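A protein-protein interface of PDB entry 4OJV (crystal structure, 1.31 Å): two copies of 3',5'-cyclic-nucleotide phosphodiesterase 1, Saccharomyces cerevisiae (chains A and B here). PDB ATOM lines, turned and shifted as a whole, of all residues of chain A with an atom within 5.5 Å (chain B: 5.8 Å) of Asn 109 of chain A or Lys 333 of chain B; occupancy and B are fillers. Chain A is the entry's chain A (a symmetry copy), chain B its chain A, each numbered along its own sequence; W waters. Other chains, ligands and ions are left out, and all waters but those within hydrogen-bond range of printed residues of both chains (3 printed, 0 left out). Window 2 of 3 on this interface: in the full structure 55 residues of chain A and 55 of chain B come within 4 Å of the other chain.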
ATOM      1  N   SER A 107     -14.265 -34.916  -2.605  1.00  0.00           N
ATOM      2  CA  SER A 107     -13.651 -34.863  -3.924  1.00  0.00           C
ATOM      3  C   SER A 107     -14.565 -34.192  -4.949  1.00  0.00           C
ATOM      4  O   SER A 107     -14.081 -33.611  -5.915  1.00  0.00           O
ATOM      5  CB  SER A 107     -13.262 -36.266  -4.402  1.00  0.00           C
ATOM      6  OG  SER A 107     -14.405 -37.060  -4.665  1.00  0.00           O
ATOM      7  N   ALA A 108     -15.882 -34.265  -4.734  1.00  0.00           N
ATOM      8  CA  ALA A 108     -16.850 -33.748  -5.702  1.00  0.00           C
ATOM      9  C   ALA A 108     -16.872 -32.228  -5.700  1.00  0.00           C
ATOM     10  O   ALA A 108     -17.041 -31.597  -4.658  1.00  0.00           O
ATOM     11  CB  ALA A 108     -18.242 -34.297  -5.418  1.00  0.00           C
ATOM     12  N   ASN A 109     -16.704 -31.626  -6.870  1.00  0.00           N
ATOM     13  CA  ASN A 109     -16.788 -30.174  -6.959  1.00  0.00           C
ATOM     14  C   ASN A 109     -18.243 -29.694  -6.884  1.00  0.00           C
ATOM     15  O   ASN A 109     -19.175 -30.506  -6.851  1.00  0.00           O
ATOM     16  CB  ASN A 109     -16.040 -29.643  -8.193  1.00  0.00           C
ATOM     17  CG  ASN A 109     -16.616 -30.134  -9.509  1.00  0.00           C
ATOM     18  OD1 ASN A 109     -17.834 -30.255  -9.670  1.00  0.00           O
ATOM     19  ND2 ASN A 109     -15.742 -30.363 -10.485  1.00  0.00           N
ATOM     20  N   THR A 110     -18.430 -28.383  -6.817  1.00  0.00           N
ATOM     21  CA  THR A 110     -19.771 -27.831  -6.635  1.00  0.00           C
ATOM     22  C   THR A 110     -20.713 -28.241  -7.767  1.00  0.00           C
ATOM     23  O   THR A 110     -21.866 -28.595  -7.518  1.00  0.00           O
ATOM     24  CB  THR A 110     -19.715 -26.305  -6.464  1.00  0.00           C
ATOM     25  OG1 THR A 110     -18.896 -26.007  -5.323  1.00  0.00           O
ATOM     26  CG2 THR A 110     -21.108 -25.737  -6.244  1.00  0.00           C
ATOM     27  N   MET A 111     -20.213 -28.222  -9.002  1.00  0.00           N
ATOM     28  CA  MET A 111     -21.026 -28.644 -10.139  1.00  0.00           C
ATOM     29  C   MET A 111     -21.482 -30.102 -10.021  1.00  0.00           C
ATOM     30  O   MET A 111     -22.658 -30.412 -10.245  1.00  0.00           O
ATOM     31  CB  MET A 111     -20.272 -28.427 -11.452  1.00  0.00           C
ATOM     32  CG  MET A 111     -21.145 -28.538 -12.693  1.00  0.00           C
ATOM     33  SD  MET A 111     -22.320 -27.176 -12.880  1.00  0.00           S
ATOM     34  CE  MET A 111     -21.219 -25.772 -12.938  1.00  0.00           C
ATOM     35  N   LYS A 112     -20.562 -30.985  -9.643  1.00  0.00           N
ATOM     36  CA  LYS A 112     -20.884 -32.392  -9.465  1.00  0.00           C
ATOM     37  C   LYS A 112     -21.914 -32.605  -8.357  1.00  0.00           C
ATOM     38  O   LYS A 112     -22.859 -33.388  -8.524  1.00  0.00           O
ATOM     39  CB  LYS A 112     -19.621 -33.204  -9.161  1.00  0.00           C
ATOM     40  CG  LYS A 112     -19.843 -34.705  -9.009  1.00  0.00           C
ATOM     41  CD  LYS A 112     -20.385 -35.321 -10.289  1.00  0.00           C
ATOM     42  CE  LYS A 112     -20.364 -36.837 -10.239  1.00  0.00           C
ATOM     43  NZ  LYS A 112     -20.967 -37.421 -11.469  1.00  0.00           N
ATOM     44  N   LYS A 113     -21.738 -31.902  -7.238  1.00  0.00           N
ATOM     45  CA  LYS A 113     -22.707 -31.984  -6.135  1.00  0.00           C
ATOM     46  C   LYS A 113     -24.098 -31.552  -6.599  1.00  0.00           C
ATOM     47  O   LYS A 113     -25.107 -32.123  -6.184  1.00  0.00           O
ATOM     48  CB  LYS A 113     -22.276 -31.111  -4.964  1.00  0.00           C
ATOM     49  CG  LYS A 113     -21.037 -31.578  -4.212  1.00  0.00           C
ATOM     50  CD  LYS A 113     -20.836 -30.701  -2.982  1.00  0.00           C
ATOM     51  CE  LYS A 113     -19.591 -31.063  -2.188  1.00  0.00           C
ATOM     52  NZ  LYS A 113     -18.387 -30.332  -2.667  1.00  0.00           N
ATOM     53  N   THR A 114     -24.136 -30.534  -7.459  1.00  0.00           N
ATOM     54  CA  THR A 114     -25.389 -30.017  -8.003  1.00  0.00           C
ATOM     55  C   THR A 114     -26.096 -31.081  -8.842  1.00  0.00           C
ATOM     56  O   THR A 114     -27.292 -31.325  -8.657  1.00  0.00           O
ATOM     57  CB  THR A 114     -25.142 -28.744  -8.839  1.00  0.00           C
ATOM     58  OG1 THR A 114     -24.522 -27.751  -8.021  1.00  0.00           O
ATOM     59  CG2 THR A 114     -26.450 -28.183  -9.379  1.00  0.00           C
ATOM     60  N   PHE B  68     -17.236 -23.048 -10.457  1.00  0.00           N
ATOM     61  CA  PHE B  68     -17.872 -24.169  -9.735  1.00  0.00           C
ATOM     62  C   PHE B  68     -17.276 -25.547 -10.035  1.00  0.00           C
ATOM     63  O   PHE B  68     -17.888 -26.578  -9.746  1.00  0.00           O
ATOM     64  CB  PHE B  68     -19.407 -24.144  -9.861  1.00  0.00           C
ATOM     65  CG  PHE B  68     -20.016 -22.828  -9.459  1.00  0.00           C
ATOM     66  CD1 PHE B  68     -19.898 -22.355  -8.153  1.00  0.00           C
ATOM     67  CD2 PHE B  68     -20.678 -22.043 -10.393  1.00  0.00           C
ATOM     68  CE1 PHE B  68     -20.444 -21.131  -7.785  1.00  0.00           C
ATOM     69  CE2 PHE B  68     -21.243 -20.828 -10.029  1.00  0.00           C
ATOM     70  CZ  PHE B  68     -21.123 -20.371  -8.725  1.00  0.00           C
ATOM     71  N   TYR B  69     -16.062 -25.558 -10.578  1.00  0.00           N
ATOM     72  CA  TYR B  69     -15.371 -26.807 -10.862  1.00  0.00           C
ATOM     73  C   TYR B  69     -14.170 -26.936  -9.924  1.00  0.00           C
ATOM     74  O   TYR B  69     -14.357 -27.032  -8.715  1.00  0.00           O
ATOM     75  CB  TYR B  69     -15.010 -26.913 -12.344  1.00  0.00           C
ATOM     76  CG  TYR B  69     -16.245 -26.991 -13.224  1.00  0.00           C
ATOM     77  CD1 TYR B  69     -16.941 -25.836 -13.610  1.00  0.00           C
ATOM     78  CD2 TYR B  69     -16.725 -28.222 -13.666  1.00  0.00           C
ATOM     79  CE1 TYR B  69     -18.076 -25.901 -14.407  1.00  0.00           C
ATOM     80  CE2 TYR B  69     -17.869 -28.301 -14.463  1.00  0.00           C
ATOM     81  CZ  TYR B  69     -18.536 -27.134 -14.828  1.00  0.00           C
ATOM     82  OH  TYR B  69     -19.663 -27.207 -15.641  1.00  0.00           O
ATOM     83  N   GLU B  70     -12.948 -26.912 -10.441  1.00  0.00           N
ATOM     84  CA  GLU B  70     -11.770 -26.964  -9.563  1.00  0.00           C
ATOM     85  C   GLU B  70     -11.848 -25.896  -8.471  1.00  0.00           C
ATOM     86  O   GLU B  70     -11.455 -26.150  -7.327  1.00  0.00           O
ATOM     87  CB  GLU B  70     -10.489 -26.857 -10.381  1.00  0.00           C
ATOM     88  CG  GLU B  70     -10.248 -28.100 -11.227  1.00  0.00           C
ATOM     89  CD  GLU B  70      -9.188 -27.906 -12.283  1.00  0.00           C
ATOM     90  OE1 GLU B  70      -9.253 -26.913 -13.030  1.00  0.00           O
ATOM     91  OE2 GLU B  70      -8.283 -28.764 -12.369  1.00  0.00           O
ATOM     92  N   PRO B 331     -20.748 -32.731 -15.584  1.00  0.00           N
ATOM     93  CA  PRO B 331     -20.236 -33.162 -14.279  1.00  0.00           C
ATOM     94  C   PRO B 331     -18.777 -33.641 -14.360  1.00  0.00           C
ATOM     95  O   PRO B 331     -18.469 -34.791 -14.039  1.00  0.00           O
ATOM     96  CB  PRO B 331     -21.194 -34.294 -13.883  1.00  0.00           C
ATOM     97  CG  PRO B 331     -21.683 -34.832 -15.181  1.00  0.00           C
ATOM     98  CD  PRO B 331     -21.733 -33.682 -16.141  1.00  0.00           C
ATOM     99  N   ALA B 332     -17.904 -32.737 -14.806  1.00  0.00           N
ATOM    100  CA  ALA B 332     -16.490 -33.008 -15.028  1.00  0.00           C
ATOM    101  C   ALA B 332     -15.640 -32.363 -13.947  1.00  0.00           C
ATOM    102  O   ALA B 332     -16.104 -31.493 -13.214  1.00  0.00           O
ATOM    103  CB  ALA B 332     -16.066 -32.493 -16.396  1.00  0.00           C
ATOM    104  N   LYS B 333     -14.383 -32.790 -13.851  1.00  0.00           N
ATOM    105  CA  LYS B 333     -13.481 -32.241 -12.848  1.00  0.00           C
ATOM    106  C   LYS B 333     -13.088 -30.803 -13.170  1.00  0.00           C
ATOM    107  O   LYS B 333     -12.937 -29.987 -12.266  1.00  0.00           O
ATOM    108  CB  LYS B 333     -12.234 -33.114 -12.696  1.00  0.00           C
ATOM    109  CG  LYS B 333     -12.507 -34.481 -12.083  1.00  0.00           C
ATOM    110  CD  LYS B 333     -11.227 -35.284 -11.901  1.00  0.00           C
ATOM    111  CE  LYS B 333     -11.507 -36.613 -11.218  1.00  0.00           C
ATOM    112  NZ  LYS B 333     -10.262 -37.391 -10.974  1.00  0.00           N
ATOM    113  N   ARG B 334     -12.944 -30.497 -14.459  1.00  0.00           N
ATOM    114  CA  ARG B 334     -12.463 -29.181 -14.895  1.00  0.00           C
ATOM    115  C   ARG B 334     -13.548 -28.416 -15.643  1.00  0.00           C
ATOM    116  O   ARG B 334     -14.337 -28.994 -16.393  1.00  0.00           O
ATOM    117  CB  ARG B 334     -11.219 -29.342 -15.774  1.00  0.00           C
ATOM    118  CG  ARG B 334     -10.491 -28.055 -16.153  1.00  0.00           C
ATOM    119  CD  ARG B 334      -8.986 -28.287 -16.252  1.00  0.00           C
ATOM    120  NE  ARG B 334      -8.240 -27.047 -16.486  1.00  0.00           N
ATOM    121  CZ  ARG B 334      -7.839 -26.617 -17.672  1.00  0.00           C
ATOM    122  NH1 ARG B 334      -8.108 -27.319 -18.767  1.00  0.00           N
ATOM    123  NH2 ARG B 334      -7.164 -25.477 -17.758  1.00  0.00           N
ATOM    124  N   ASP B 335     -13.562 -27.108 -15.428  1.00  0.00           N
ATOM    125  CA  ASP B 335     -14.492 -26.205 -16.098  1.00  0.00           C
ATOM    126  C   ASP B 335     -14.406 -26.425 -17.611  1.00  0.00           C
ATOM    127  O   ASP B 335     -13.336 -26.264 -18.205  1.00  0.00           O
ATOM    128  CB  ASP B 335     -14.111 -24.772 -15.714  1.00  0.00           C
ATOM    129  CG  ASP B 335     -15.148 -23.723 -16.112  1.00  0.00           C
ATOM    130  OD1 ASP B 335     -15.731 -23.798 -17.217  1.00  0.00           O
ATOM    131  OD2 ASP B 335     -15.337 -22.793 -15.297  1.00  0.00           O
HETATM  132  O   HOH W   1     -16.145 -26.395  -6.760  1.00  0.00           O
HETATM  133  O   HOH W   2     -12.959 -30.797  -9.665  1.00  0.00           O
HETATM  134  O   HOH W   3     -18.621 -31.777 -12.001  1.00  0.00           O
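OD1 of Asn 109 of chain A lies within hydrogen-bond range of N of Met 111 of chain A (3.2 Å). The side-chain amide oxygen (OD1) of Asn 109 of chain A sits at hydrogen-bond distance from the backbone NH (N) of Lys 112 of chain A (2.8 Å). The side-chain hydroxyl (OG1) of Thr 114 of chain A lies within hydrogen-bond range of the backbone carbonyl oxygen (O) of Thr 110 of chain A, 2.8 Å away.
No position is printed for both chains.
Of chain A, only Asn 109 comes within 4 Å of Lys 333 of chain B. Printed residues of chain A within 4 Å of Ala 332 of chain B: Asn 109 (3.0 Å). Printed residues of chain A within 4 Å of Pro 331 of chain B: Lys 112 (3.8 Å). Printed residues of chain B within 4 Å of Thr 110 of chain A: Phe 68. Printed residues of chain A within 4 Å of Tyr 69 of chain B: Asn 109 and Met 111. Of the printed residues of chain B, Lys 112 of chain A touches Pro 331 (3.8 Å). Thr 114 of chain A touches none of the printed residues of chain B. Arg 334 of chain B touches none of the printed residues of chain A. The nearest printed residue of chain A that does not touch Ala 332 of chain B is Met 111 of chain A (5.5 Å).
Printed residues of chain B that touch a printed residue of chain A: Phe 68, Tyr 69, Pro 331, Ala 332 and Lys 333. Hydrophobic or aromatic side chains of chain B within 4 Å of the printed part of chain A: Phe 68, Tyr 69 and Pro 331. Along chain B the printed residues that touch a printed residue of chain A span positions 68 to 333. Among the printed residues, 8 pairs touch across the chains.
N of Thr 110 of chain A lies within hydrogen-bond range of O of Phe 68 of chain B (3.5 Å). The backbone carbonyl oxygen (O) of Phe 68 of chain B sits at hydrogen-bond distance from the backbone NH (N) of Met 111 of chain A (2.9 Å). The side-chain amide nitrogen (ND2) of Asn 109 of chain A is in hydrogen-bond range of the backbone carbonyl oxygen (O) of Ala 332 of chain B, at 3.0 Å. The backbone carbonyl oxygen (O) of Lys 333 of chain B lies within hydrogen-bond range of the side-chain amide nitrogen (ND2) of Asn 109 of chain A, at 3.3 Å.
Water W2 bridges O of Lys 333 of chain B and ND2 of Asn 109 of chain A. Water W1 lies within hydrogen-bond range of O of Tyr 69 of chain B (2.7 Å), N of Thr 110 of chain A (3.0 Å) and O of Phe 68 of chain B (3.5 Å). Water W3 lies within hydrogen-bond range of O of Ala 332 of chain B, OD1 of Asn 109 of chain A and N of Lys 112 of chain A.
Among the printed residues, pairs that only touch across the chains: Asn 109 of chain A with Tyr 69 of chain B (3.1 Å), Met 111 of chain A with Tyr 69 of chain B (3.4 Å), Asn 109 of chain A with Phe 68 of chain B (3.7 Å) and Lys 112 of chain A with Pro 331 of chain B (3.8 Å).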
